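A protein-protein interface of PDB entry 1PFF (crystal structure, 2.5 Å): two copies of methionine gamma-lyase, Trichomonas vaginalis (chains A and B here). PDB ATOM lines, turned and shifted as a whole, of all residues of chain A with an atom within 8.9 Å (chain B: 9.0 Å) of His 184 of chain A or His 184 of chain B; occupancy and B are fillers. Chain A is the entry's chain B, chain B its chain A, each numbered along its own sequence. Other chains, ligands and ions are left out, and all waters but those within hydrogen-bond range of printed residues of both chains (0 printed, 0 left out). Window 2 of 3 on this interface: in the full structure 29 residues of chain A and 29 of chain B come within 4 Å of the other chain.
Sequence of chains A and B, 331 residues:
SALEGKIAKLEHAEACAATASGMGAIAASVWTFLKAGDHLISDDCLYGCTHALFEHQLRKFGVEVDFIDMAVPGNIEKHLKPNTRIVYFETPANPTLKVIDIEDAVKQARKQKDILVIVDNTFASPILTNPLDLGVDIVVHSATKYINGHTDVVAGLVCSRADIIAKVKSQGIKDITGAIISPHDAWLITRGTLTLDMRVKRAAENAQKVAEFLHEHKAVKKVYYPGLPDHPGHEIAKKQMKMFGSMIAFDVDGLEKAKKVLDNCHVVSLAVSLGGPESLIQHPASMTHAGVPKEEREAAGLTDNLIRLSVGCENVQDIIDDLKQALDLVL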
ATOM      1  N   LEU A   3      21.280 -38.374  -4.303  1.00  0.00           N
ATOM      2  CA  LEU A   3      22.592 -37.759  -4.176  1.00  0.00           C
ATOM      3  C   LEU A   3      23.506 -38.633  -3.314  1.00  0.00           C
ATOM      4  O   LEU A   3      24.644 -38.907  -3.684  1.00  0.00           O
ATOM      5  CB  LEU A   3      22.481 -36.360  -3.567  1.00  0.00           C
ATOM      6  CG  LEU A   3      23.762 -35.713  -3.019  1.00  0.00           C
ATOM      7  CD1 LEU A   3      24.782 -35.469  -4.126  1.00  0.00           C
ATOM      8  CD2 LEU A   3      23.433 -34.410  -2.289  1.00  0.00           C
ATOM      9  N   ASN A 148      29.883 -29.631  -6.124  1.00  0.00           N
ATOM     10  CA  ASN A 148      28.722 -28.790  -6.447  1.00  0.00           C
ATOM     11  C   ASN A 148      28.539 -28.452  -7.933  1.00  0.00           C
ATOM     12  O   ASN A 148      27.414 -28.220  -8.386  1.00  0.00           O
ATOM     13  CB  ASN A 148      28.704 -27.511  -5.587  1.00  0.00           C
ATOM     14  CG  ASN A 148      29.899 -26.598  -5.843  1.00  0.00           C
ATOM     15  OD1 ASN A 148      30.802 -26.915  -6.621  1.00  0.00           O
ATOM     16  ND2 ASN A 148      29.902 -25.449  -5.177  1.00  0.00           N
ATOM     17  N   HIS A 150      29.220 -25.786  -9.747  1.00  0.00           N
ATOM     18  CA  HIS A 150      28.710 -24.440 -10.068  1.00  0.00           C
ATOM     19  C   HIS A 150      29.147 -23.400  -9.025  1.00  0.00           C
ATOM     20  O   HIS A 150      29.954 -22.519  -9.334  1.00  0.00           O
ATOM     21  CB  HIS A 150      27.176 -24.429 -10.228  1.00  0.00           C
ATOM     22  CG  HIS A 150      26.439 -25.132  -9.126  1.00  0.00           C
ATOM     23  ND1 HIS A 150      25.125 -25.535  -9.247  1.00  0.00           N
ATOM     24  CD2 HIS A 150      26.830 -25.499  -7.881  1.00  0.00           C
ATOM     25  CE1 HIS A 150      24.742 -26.120  -8.127  1.00  0.00           C
ATOM     26  NE2 HIS A 150      25.759 -26.116  -7.282  1.00  0.00           N
ATOM     27  N   ASP A 152      27.816 -20.825  -5.367  1.00  0.00           N
ATOM     28  CA  ASP A 152      26.757 -20.190  -4.564  1.00  0.00           C
ATOM     29  C   ASP A 152      26.002 -21.227  -3.724  1.00  0.00           C
ATOM     30  O   ASP A 152      24.985 -20.927  -3.081  1.00  0.00           O
ATOM     31  CB  ASP A 152      25.795 -19.351  -5.418  1.00  0.00           C
ATOM     32  CG  ASP A 152      25.200 -18.184  -4.649  1.00  0.00           C
ATOM     33  OD1 ASP A 152      25.499 -18.046  -3.438  1.00  0.00           O
ATOM     34  OD2 ASP A 152      24.422 -17.354  -5.171  1.00  0.00           O
ATOM     35  N   VAL A 153      26.530 -22.445  -3.726  1.00  0.00           N
ATOM     36  CA  VAL A 153      25.870 -23.586  -3.111  1.00  0.00           C
ATOM     37  C   VAL A 153      26.786 -24.192  -2.057  1.00  0.00           C
ATOM     38  O   VAL A 153      27.903 -24.627  -2.348  1.00  0.00           O
ATOM     39  CB  VAL A 153      25.479 -24.629  -4.179  1.00  0.00           C
ATOM     40  CG1 VAL A 153      24.979 -25.920  -3.546  1.00  0.00           C
ATOM     41  CG2 VAL A 153      24.427 -24.046  -5.114  1.00  0.00           C
ATOM     42  N   VAL A 154      26.301 -24.208  -0.826  1.00  0.00           N
ATOM     43  CA  VAL A 154      27.067 -24.734   0.293  1.00  0.00           C
ATOM     44  C   VAL A 154      26.385 -26.019   0.778  1.00  0.00           C
ATOM     45  O   VAL A 154      25.164 -26.082   0.924  1.00  0.00           O
ATOM     46  CB  VAL A 154      27.250 -23.655   1.409  1.00  0.00           C
ATOM     47  CG1 VAL A 154      28.039 -24.188   2.597  1.00  0.00           C
ATOM     48  CG2 VAL A 154      27.948 -22.414   0.840  1.00  0.00           C
ATOM     49  N   ALA A 155      27.184 -27.063   0.951  1.00  0.00           N
ATOM     50  CA  ALA A 155      26.690 -28.370   1.371  1.00  0.00           C
ATOM     51  C   ALA A 155      27.888 -29.190   1.793  1.00  0.00           C
ATOM     52  O   ALA A 155      29.019 -28.871   1.425  1.00  0.00           O
ATOM     53  CB  ALA A 155      25.951 -29.066   0.232  1.00  0.00           C
ATOM     54  N   ILE A 181      20.746 -30.725   4.738  1.00  0.00           N
ATOM     55  CA  ILE A 181      20.901 -30.138   3.398  1.00  0.00           C
ATOM     56  C   ILE A 181      19.563 -29.649   2.833  1.00  0.00           C
ATOM     57  O   ILE A 181      18.516 -30.270   3.061  1.00  0.00           O
ATOM     58  CB  ILE A 181      21.633 -31.112   2.410  1.00  0.00           C
ATOM     59  CG1 ILE A 181      22.155 -30.343   1.184  1.00  0.00           C
ATOM     60  CG2 ILE A 181      20.743 -32.316   1.993  1.00  0.00           C
ATOM     61  CD1 ILE A 181      23.124 -31.125   0.313  1.00  0.00           C
ATOM     62  N   SER A 182      19.608 -28.536   2.100  1.00  0.00           N
ATOM     63  CA  SER A 182      18.441 -28.044   1.374  1.00  0.00           C
ATOM     64  C   SER A 182      18.132 -28.961   0.187  1.00  0.00           C
ATOM     65  O   SER A 182      19.049 -29.368  -0.532  1.00  0.00           O
ATOM     66  CB  SER A 182      18.692 -26.614   0.882  1.00  0.00           C
ATOM     67  OG  SER A 182      17.857 -26.283  -0.214  1.00  0.00           O
ATOM     68  N   PRO A 183      16.854 -29.296  -0.009  1.00  0.00           N
ATOM     69  CA  PRO A 183      16.415 -30.058  -1.190  1.00  0.00           C
ATOM     70  C   PRO A 183      16.903 -29.421  -2.490  1.00  0.00           C
ATOM     71  O   PRO A 183      17.276 -30.126  -3.429  1.00  0.00           O
ATOM     72  CB  PRO A 183      14.883 -29.964  -1.112  1.00  0.00           C
ATOM     73  CG  PRO A 183      14.592 -29.813   0.342  1.00  0.00           C
ATOM     74  CD  PRO A 183      15.733 -28.991   0.900  1.00  0.00           C
ATOM     75  N   HIS A 184      16.917 -28.092  -2.524  1.00  0.00           N
ATOM     76  CA  HIS A 184      17.334 -27.338  -3.703  1.00  0.00           C
ATOM     77  C   HIS A 184      18.838 -27.437  -3.973  1.00  0.00           C
ATOM     78  O   HIS A 184      19.261 -27.641  -5.113  1.00  0.00           O
ATOM     79  CB  HIS A 184      16.869 -25.894  -3.564  1.00  0.00           C
ATOM     80  CG  HIS A 184      15.398 -25.772  -3.307  1.00  0.00           C
ATOM     81  ND1 HIS A 184      14.874 -25.558  -2.048  1.00  0.00           N
ATOM     82  CD2 HIS A 184      14.336 -25.862  -4.146  1.00  0.00           C
ATOM     83  CE1 HIS A 184      13.555 -25.506  -2.126  1.00  0.00           C
ATOM     84  NE2 HIS A 184      13.203 -25.691  -3.386  1.00  0.00           N
ATOM     85  N   ASP A 185      19.638 -27.315  -2.917  1.00  0.00           N
ATOM     86  CA  ASP A 185      21.086 -27.471  -3.023  1.00  0.00           C
ATOM     87  C   ASP A 185      21.478 -28.918  -3.336  1.00  0.00           C
ATOM     88  O   ASP A 185      22.408 -29.157  -4.108  1.00  0.00           O
ATOM     89  CB  ASP A 185      21.771 -26.962  -1.753  1.00  0.00           C
ATOM     90  CG  ASP A 185      21.683 -25.446  -1.614  1.00  0.00           C
ATOM     91  OD1 ASP A 185      22.586 -24.851  -0.999  1.00  0.00           O
ATOM     92  OD2 ASP A 185      20.753 -24.762  -2.089  1.00  0.00           O
ATOM     93  N   ALA A 186      20.745 -29.874  -2.764  1.00  0.00           N
ATOM     94  CA  ALA A 186      20.966 -31.296  -3.048  1.00  0.00           C
ATOM     95  C   ALA A 186      20.766 -31.623  -4.541  1.00  0.00           C
ATOM     96  O   ALA A 186      21.538 -32.394  -5.126  1.00  0.00           O
ATOM     97  CB  ALA A 186      20.067 -32.168  -2.173  1.00  0.00           C
ATOM     98  N   TRP A 187      19.745 -31.019  -5.146  1.00  0.00           N
ATOM     99  CA  TRP A 187      19.477 -31.178  -6.582  1.00  0.00           C
ATOM    100  C   TRP A 187      20.664 -30.662  -7.395  1.00  0.00           C
ATOM    101  O   TRP A 187      21.138 -31.326  -8.318  1.00  0.00           O
ATOM    102  CB  TRP A 187      18.201 -30.425  -6.967  1.00  0.00           C
ATOM    103  CG  TRP A 187      17.770 -30.627  -8.398  1.00  0.00           C
ATOM    104  CD1 TRP A 187      16.917 -31.589  -8.873  1.00  0.00           C
ATOM    105  CD2 TRP A 187      18.166 -29.850  -9.536  1.00  0.00           C
ATOM    106  NE1 TRP A 187      16.757 -31.454 -10.231  1.00  0.00           N
ATOM    107  CE2 TRP A 187      17.514 -30.399 -10.668  1.00  0.00           C
ATOM    108  CE3 TRP A 187      19.005 -28.743  -9.719  1.00  0.00           C
ATOM    109  CZ2 TRP A 187      17.678 -29.878 -11.959  1.00  0.00           C
ATOM    110  CZ3 TRP A 187      19.168 -28.226 -11.010  1.00  0.00           C
ATOM    111  CH2 TRP A 187      18.508 -28.797 -12.108  1.00  0.00           C
ATOM    112  N   LEU A 188      21.144 -29.480  -7.019  1.00  0.00           N
ATOM    113  CA  LEU A 188      22.279 -28.839  -7.671  1.00  0.00           C
ATOM    114  C   LEU A 188      23.605 -29.608  -7.510  1.00  0.00           C
ATOM    115  O   LEU A 188      24.409 -29.669  -8.446  1.00  0.00           O
ATOM    116  CB  LEU A 188      22.404 -27.393  -7.177  1.00  0.00           C
ATOM    117  CG  LEU A 188      21.303 -26.418  -7.628  1.00  0.00           C
ATOM    118  CD1 LEU A 188      21.339 -25.133  -6.812  1.00  0.00           C
ATOM    119  CD2 LEU A 188      21.405 -26.098  -9.111  1.00  0.00           C
ATOM    120  N   ILE A 189      23.832 -30.200  -6.340  1.00  0.00           N
ATOM    121  CA  ILE A 189      25.004 -31.065  -6.156  1.00  0.00           C
ATOM    122  C   ILE A 189      24.922 -32.287  -7.080  1.00  0.00           C
ATOM    123  O   ILE A 189      25.924 -32.680  -7.690  1.00  0.00           O
ATOM    124  CB  ILE A 189      25.176 -31.522  -4.677  1.00  0.00           C
ATOM    125  CG1 ILE A 189      25.125 -30.343  -3.690  1.00  0.00           C
ATOM    126  CG2 ILE A 189      26.464 -32.327  -4.505  1.00  0.00           C
ATOM    127  CD1 ILE A 189      26.275 -29.368  -3.778  1.00  0.00           C
ATOM    128  N   THR A 190      23.722 -32.869  -7.174  1.00  0.00           N
ATOM    129  CA  THR A 190      23.458 -34.058  -7.992  1.00  0.00           C
ATOM    130  C   THR A 190      23.739 -33.771  -9.466  1.00  0.00           C
ATOM    131  O   THR A 190      24.296 -34.602 -10.179  1.00  0.00           O
ATOM    132  CB  THR A 190      21.993 -34.528  -7.801  1.00  0.00           C
ATOM    133  OG1 THR A 190      21.737 -34.735  -6.407  1.00  0.00           O
ATOM    134  CG2 THR A 190      21.777 -35.915  -8.399  1.00  0.00           C
ATOM    135  N   ARG A 191      23.338 -32.582  -9.900  1.00  0.00           N
ATOM    136  CA  ARG A 191      23.624 -32.070 -11.235  1.00  0.00           C
ATOM    137  C   ARG A 191      25.136 -31.998 -11.473  1.00  0.00           C
ATOM    138  O   ARG A 191      25.620 -32.421 -12.520  1.00  0.00           O
ATOM    139  CB  ARG A 191      22.979 -30.688 -11.382  1.00  0.00           C
ATOM    140  CG  ARG A 191      23.159 -30.015 -12.726  1.00  0.00           C
ATOM    141  CD  ARG A 191      22.786 -28.544 -12.691  1.00  0.00           C
ATOM    142  NE  ARG A 191      22.597 -27.990 -14.029  1.00  0.00           N
ATOM    143  CZ  ARG A 191      23.448 -27.166 -14.630  1.00  0.00           C
ATOM    144  NH1 ARG A 191      24.570 -26.796 -14.026  1.00  0.00           N
ATOM    145  NH2 ARG A 191      23.177 -26.713 -15.846  1.00  0.00           N
ATOM    146  N   LEU B   3      16.940 -11.311   4.743  1.00  0.00           N
ATOM    147  CA  LEU B   3      16.035 -12.180   5.487  1.00  0.00           C
ATOM    148  C   LEU B   3      16.149 -11.895   6.978  1.00  0.00           C
ATOM    149  O   LEU B   3      15.141 -11.682   7.660  1.00  0.00           O
ATOM    150  CB  LEU B   3      16.318 -13.664   5.209  1.00  0.00           C
ATOM    151  CG  LEU B   3      15.546 -14.698   6.059  1.00  0.00           C
ATOM    152  CD1 LEU B   3      14.036 -14.594   5.879  1.00  0.00           C
ATOM    153  CD2 LEU B   3      16.017 -16.125   5.779  1.00  0.00           C
ATOM    154  N   ASN B 148       7.844 -19.715   5.949  1.00  0.00           N
ATOM    155  CA  ASN B 148       7.821 -20.151   4.549  1.00  0.00           C
ATOM    156  C   ASN B 148       6.392 -20.326   4.034  1.00  0.00           C
ATOM    157  O   ASN B 148       5.524 -20.820   4.752  1.00  0.00           O
ATOM    158  CB  ASN B 148       8.577 -21.471   4.366  1.00  0.00           C
ATOM    159  CG  ASN B 148       8.700 -21.878   2.898  1.00  0.00           C
ATOM    160  OD1 ASN B 148       9.100 -21.079   2.055  1.00  0.00           O
ATOM    161  ND2 ASN B 148       8.345 -23.118   2.592  1.00  0.00           N
ATOM    162  N   HIS B 150       5.205 -22.394   1.881  1.00  0.00           N
ATOM    163  CA  HIS B 150       4.954 -23.740   1.350  1.00  0.00           C
ATOM    164  C   HIS B 150       5.521 -24.790   2.328  1.00  0.00           C
ATOM    165  O   HIS B 150       5.816 -24.468   3.477  1.00  0.00           O
ATOM    166  CB  HIS B 150       5.575 -23.858  -0.056  1.00  0.00           C
ATOM    167  CG  HIS B 150       5.121 -25.058  -0.838  1.00  0.00           C
ATOM    168  ND1 HIS B 150       3.836 -25.174  -1.359  1.00  0.00           N
ATOM    169  CD2 HIS B 150       5.790 -26.189  -1.195  1.00  0.00           C
ATOM    170  CE1 HIS B 150       3.730 -26.328  -1.997  1.00  0.00           C
ATOM    171  NE2 HIS B 150       4.903 -26.963  -1.912  1.00  0.00           N
ATOM    172  N   THR B 151       5.661 -26.036   1.876  1.00  0.00           N
ATOM    173  CA  THR B 151       6.214 -27.123   2.694  1.00  0.00           C
ATOM    174  C   THR B 151       7.543 -27.669   2.144  1.00  0.00           C
ATOM    175  O   THR B 151       7.983 -28.758   2.532  1.00  0.00           O
ATOM    176  CB  THR B 151       5.194 -28.288   2.799  1.00  0.00           C
ATOM    177  OG1 THR B 151       4.720 -28.632   1.491  1.00  0.00           O
ATOM    178  CG2 THR B 151       3.933 -27.856   3.537  1.00  0.00           C
ATOM    179  N   ASP B 152       8.179 -26.914   1.248  1.00  0.00           N
ATOM    180  CA  ASP B 152       9.338 -27.397   0.496  1.00  0.00           C
ATOM    181  C   ASP B 152      10.693 -26.879   1.002  1.00  0.00           C
ATOM    182  O   ASP B 152      11.725 -27.087   0.351  1.00  0.00           O
ATOM    183  CB  ASP B 152       9.176 -27.034  -0.985  1.00  0.00           C
ATOM    184  CG  ASP B 152       9.098 -25.527  -1.216  1.00  0.00           C
ATOM    185  OD1 ASP B 152       8.658 -24.793  -0.308  1.00  0.00           O
ATOM    186  OD2 ASP B 152       9.456 -24.986  -2.277  1.00  0.00           O
ATOM    187  N   VAL B 153      10.690 -26.202   2.147  1.00  0.00           N
ATOM    188  CA  VAL B 153      11.917 -25.619   2.692  1.00  0.00           C
ATOM    189  C   VAL B 153      12.175 -26.103   4.116  1.00  0.00           C
ATOM    190  O   VAL B 153      11.247 -26.247   4.910  1.00  0.00           O
ATOM    191  CB  VAL B 153      11.876 -24.062   2.670  1.00  0.00           C
ATOM    192  CG1 VAL B 153      12.938 -23.476   3.576  1.00  0.00           C
ATOM    193  CG2 VAL B 153      12.038 -23.523   1.256  1.00  0.00           C
ATOM    194  N   VAL B 154      13.448 -26.358   4.415  1.00  0.00           N
ATOM    195  CA  VAL B 154      13.925 -26.570   5.779  1.00  0.00           C
ATOM    196  C   VAL B 154      14.845 -25.401   6.115  1.00  0.00           C
ATOM    197  O   VAL B 154      15.805 -25.122   5.386  1.00  0.00           O
ATOM    198  CB  VAL B 154      14.692 -27.899   5.940  1.00  0.00           C
ATOM    199  CG1 VAL B 154      14.682 -28.352   7.401  1.00  0.00           C
ATOM    200  CG2 VAL B 154      14.099 -28.971   5.043  1.00  0.00           C
ATOM    201  N   ALA B 155      14.523 -24.701   7.198  1.00  0.00           N
ATOM    202  CA  ALA B 155      15.268 -23.518   7.617  1.00  0.00           C
ATOM    203  C   ALA B 155      14.887 -23.173   9.048  1.00  0.00           C
ATOM    204  O   ALA B 155      13.808 -23.543   9.515  1.00  0.00           O
ATOM    205  CB  ALA B 155      14.968 -22.334   6.705  1.00  0.00           C
ATOM    206  N   ILE B 181      22.152 -21.723   6.373  1.00  0.00           N
ATOM    207  CA  ILE B 181      20.974 -21.720   5.491  1.00  0.00           C
ATOM    208  C   ILE B 181      21.387 -21.670   4.016  1.00  0.00           C
ATOM    209  O   ILE B 181      22.373 -21.023   3.658  1.00  0.00           O
ATOM    210  CB  ILE B 181      20.006 -20.530   5.834  1.00  0.00           C
ATOM    211  CG1 ILE B 181      18.613 -20.776   5.236  1.00  0.00           C
ATOM    212  CG2 ILE B 181      20.587 -19.186   5.386  1.00  0.00           C
ATOM    213  CD1 ILE B 181      17.535 -19.752   5.645  1.00  0.00           C
ATOM    214  N   SER B 182      20.634 -22.369   3.169  1.00  0.00           N
ATOM    215  CA  SER B 182      20.805 -22.259   1.726  1.00  0.00           C
ATOM    216  C   SER B 182      20.322 -20.883   1.274  1.00  0.00           C
ATOM    217  O   SER B 182      19.254 -20.443   1.685  1.00  0.00           O
ATOM    218  CB  SER B 182      20.003 -23.353   1.023  1.00  0.00           C
ATOM    219  OG  SER B 182      19.782 -23.032  -0.337  1.00  0.00           O
ATOM    220  N   PRO B 183      21.111 -20.187   0.453  1.00  0.00           N
ATOM    221  CA  PRO B 183      20.674 -18.907  -0.118  1.00  0.00           C
ATOM    222  C   PRO B 183      19.377 -19.027  -0.923  1.00  0.00           C
ATOM    223  O   PRO B 183      18.639 -18.045  -0.973  1.00  0.00           O
ATOM    224  CB  PRO B 183      21.838 -18.503  -1.027  1.00  0.00           C
ATOM    225  CG  PRO B 183      22.605 -19.759  -1.244  1.00  0.00           C
ATOM    226  CD  PRO B 183      22.480 -20.538   0.033  1.00  0.00           C
ATOM    227  N   HIS B 184      19.106 -20.188  -1.524  1.00  0.00           N
ATOM    228  CA  HIS B 184      17.844 -20.386  -2.245  1.00  0.00           C
ATOM    229  C   HIS B 184      16.661 -20.490  -1.278  1.00  0.00           C
ATOM    230  O   HIS B 184      15.605 -19.911  -1.511  1.00  0.00           O
ATOM    231  CB  HIS B 184      17.883 -21.619  -3.150  1.00  0.00           C
ATOM    232  CG  HIS B 184      16.606 -21.850  -3.903  1.00  0.00           C
ATOM    233  ND1 HIS B 184      16.331 -21.243  -5.111  1.00  0.00           N
ATOM    234  CD2 HIS B 184      15.515 -22.597  -3.604  1.00  0.00           C
ATOM    235  CE1 HIS B 184      15.135 -21.618  -5.531  1.00  0.00           C
ATOM    236  NE2 HIS B 184      14.620 -22.441  -4.635  1.00  0.00           N
ATOM    237  N   ASP B 185      16.845 -21.254  -0.206  1.00  0.00           N
ATOM    238  CA  ASP B 185      15.819 -21.371   0.821  1.00  0.00           C
ATOM    239  C   ASP B 185      15.591 -20.006   1.469  1.00  0.00           C
ATOM    240  O   ASP B 185      14.449 -19.607   1.675  1.00  0.00           O
ATOM    241  CB  ASP B 185      16.196 -22.442   1.854  1.00  0.00           C
ATOM    242  CG  ASP B 185      16.042 -23.860   1.311  1.00  0.00           C
ATOM    243  OD1 ASP B 185      15.969 -24.807   2.108  1.00  0.00           O
ATOM    244  OD2 ASP B 185      15.972 -24.133   0.102  1.00  0.00           O
ATOM    245  N   ALA B 186      16.675 -19.285   1.745  1.00  0.00           N
ATOM    246  CA  ALA B 186      16.597 -17.955   2.354  1.00  0.00           C
ATOM    247  C   ALA B 186      15.778 -16.987   1.504  1.00  0.00           C
ATOM    248  O   ALA B 186      14.976 -16.217   2.026  1.00  0.00           O
ATOM    249  CB  ALA B 186      17.986 -17.393   2.590  1.00  0.00           C
ATOM    250  N   TRP B 187      15.996 -17.029   0.192  1.00  0.00           N
ATOM    251  CA  TRP B 187      15.274 -16.157  -0.728  1.00  0.00           C
ATOM    252  C   TRP B 187      13.775 -16.465  -0.688  1.00  0.00           C
ATOM    253  O   TRP B 187      12.955 -15.553  -0.536  1.00  0.00           O
ATOM    254  CB  TRP B 187      15.854 -16.288  -2.141  1.00  0.00           C
ATOM    255  CG  TRP B 187      14.989 -15.723  -3.211  1.00  0.00           C
ATOM    256  CD1 TRP B 187      14.644 -14.413  -3.386  1.00  0.00           C
ATOM    257  CD2 TRP B 187      14.341 -16.453  -4.252  1.00  0.00           C
ATOM    258  NE1 TRP B 187      13.822 -14.285  -4.480  1.00  0.00           N
ATOM    259  CE2 TRP B 187      13.620 -15.522  -5.031  1.00  0.00           C
ATOM    260  CE3 TRP B 187      14.299 -17.809  -4.614  1.00  0.00           C
ATOM    261  CZ2 TRP B 187      12.864 -15.898  -6.147  1.00  0.00           C
ATOM    262  CZ3 TRP B 187      13.548 -18.186  -5.727  1.00  0.00           C
ATOM    263  CH2 TRP B 187      12.840 -17.229  -6.479  1.00  0.00           C
ATOM    264  N   LEU B 188      13.434 -17.750  -0.789  1.00  0.00           N
ATOM    265  CA  LEU B 188      12.053 -18.225  -0.674  1.00  0.00           C
ATOM    266  C   LEU B 188      11.397 -17.849   0.651  1.00  0.00           C
ATOM    267  O   LEU B 188      10.222 -17.474   0.679  1.00  0.00           O
ATOM    268  CB  LEU B 188      11.982 -19.746  -0.872  1.00  0.00           C
ATOM    269  CG  LEU B 188      12.088 -20.278  -2.306  1.00  0.00           C
ATOM    270  CD1 LEU B 188      12.046 -21.807  -2.342  1.00  0.00           C
ATOM    271  CD2 LEU B 188      11.000 -19.677  -3.202  1.00  0.00           C
ATOM    272  N   ILE B 189      12.153 -17.950   1.745  1.00  0.00           N
ATOM    273  CA  ILE B 189      11.639 -17.565   3.060  1.00  0.00           C
ATOM    274  C   ILE B 189      11.353 -16.067   3.095  1.00  0.00           C
ATOM    275  O   ILE B 189      10.312 -15.646   3.613  1.00  0.00           O
ATOM    276  CB  ILE B 189      12.627 -17.953   4.196  1.00  0.00           C
ATOM    277  CG1 ILE B 189      12.935 -19.455   4.184  1.00  0.00           C
ATOM    278  CG2 ILE B 189      12.080 -17.539   5.562  1.00  0.00           C
ATOM    279  CD1 ILE B 189      11.742 -20.341   4.382  1.00  0.00           C
ATOM    280  N   THR B 190      12.283 -15.279   2.546  1.00  0.00           N
ATOM    281  CA  THR B 190      12.137 -13.824   2.447  1.00  0.00           C
ATOM    282  C   THR B 190      10.846 -13.444   1.712  1.00  0.00           C
ATOM    283  O   THR B 190      10.153 -12.519   2.117  1.00  0.00           O
ATOM    284  CB  THR B 190      13.374 -13.186   1.749  1.00  0.00           C
ATOM    285  OG1 THR B 190      14.523 -13.320   2.595  1.00  0.00           O
ATOM    286  CG2 THR B 190      13.224 -11.669   1.615  1.00  0.00           C
ATOM    287  N   ARG B 191      10.536 -14.170   0.641  1.00  0.00           N
ATOM    288  CA  ARG B 191       9.302 -13.955  -0.117  1.00  0.00           C
ATOM    289  C   ARG B 191       8.084 -14.394   0.699  1.00  0.00           C
ATOM    290  O   ARG B 191       7.020 -13.760   0.643  1.00  0.00           O
ATOM    291  CB  ARG B 191       9.351 -14.700  -1.449  1.00  0.00           C
ATOM    292  CG  ARG B 191      10.432 -14.204  -2.425  1.00  0.00           C
ATOM    293  CD  ARG B 191      10.523 -12.678  -2.580  1.00  0.00           C
ATOM    294  NE  ARG B 191       9.443 -12.134  -3.410  1.00  0.00           N
ATOM    295  CZ  ARG B 191       9.366 -10.868  -3.825  1.00  0.00           C
ATOM    296  NH1 ARG B 191      10.306  -9.987  -3.502  1.00  0.00           N
ATOM    297  NH2 ARG B 191       8.342 -10.479  -4.567  1.00  0.00           N
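OD2 of Asp 185 of chain A is in hydrogen-bond range of OG of Ser 182 of chain B (2.6 Å).
OD2 of Asp 185 of chain B sits at hydrogen-bond distance from OG of Ser 182 of chain A (2.9 Å).
A ring nitrogen (ND1) of His 184 of chain A is in hydrogen-bond range of the side-chain carboxylate (OD2) of Asp 185 of chain B, at 2.8 Å.
The side-chain carboxylate (OD1) of Asp 152 of chain B is in hydrogen-bond range of the side-chain amide nitrogen (ND2) of Asn 148 of chain B (3.4 Å).
OG of Ser 182 of chain B sits close to N of His 184 of chain B (3.2 Å).
The backbone NH of Asp 185 of chain B lies within hydrogen-bond range of the side-chain hydroxyl of Ser 182 of chain B (3.4 Å).
The side-chain hydroxyl (OG) of Ser 182 of chain A lies within hydrogen-bond range of the backbone NH (N) of His 184 of chain A, 3.1 Å away.
The side-chain hydroxyl (OG) of Ser 182 of chain A is in hydrogen-bond range of the backbone NH (N) of Asp 185 of chain A, at 3.4 Å.
Pro 183 of chain B touches Asp 152 of chain A (CG to O, 3.2 Å).
Ser 182 of chain A touches Ser 182 of chain B.
Asp 152 of chain B touches Pro 183 of chain A (O to CG, 3.96 Å).
His 184 of chain A touches Asp 152 of chain B.
CD2 of His 184 of chain B touches CG of His 184 of chain A, 3.2 Å away.
Of the printed residues of chain B, Asp 152 of chain A touches Pro 183 (3.2 Å).
Of the printed residues of chain B, Ser 182 of chain A touches Ser 182 and Asp 185.
Of chain B, only Asp 152 (3.96 Å) comes within 4 Å of Pro 183 of chain A.
Ile 189 of chain A touches none of the printed residues of chain B.
Of chain A, only His 184 (3.2 Å) comes within 4 Å of His 184 of chain B.
Of chain A, only Ser 182 and His 184 come within 4 Å of Asp 185 of chain B.
The nearest printed residue of chain B that does not touch His 184 of chain A is Leu 188 of chain B (4.001 Å).
Of the 19 printed residues of chain B, 5 touch a printed residue of chain A.
Along chain B the printed residues that touch a printed residue of chain A span positions 152 to 185.
Of the 18 printed residues of chain A, 5 touch a printed residue of chain B.
Printed residues of chain A that touch a printed residue of chain B: Asp 152, Ser 182, Pro 183, His 184 and Asp 185.
Among the printed residues, 8 pairs touch across the chains.
Asp 152 of chain A touches Pro 183 of chain B, and with the chains exchanged Pro 183 of chain A touches Asp 152 of chain B.
Ser 182 of chain B touches its own counterpart, Ser 182 of chain A.
His 184 of chain B touches its own counterpart, His 184 of chain A.
His 184 of chain A touches Asp 185 of chain B, but with the chains exchanged Asp 185 of chain A does not touch His 184 of chain B (4.4 Å).
Positions printed for both chains: 3, 148, 150, 152, 153, 154, 155, 181, 182, 183, 184, 185, 186, 187, 188, 189, 190 and 191.
Of the 8 pairs that touch across the chains among the printed residues, 6 have their exchanged pair printed and touching as well.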
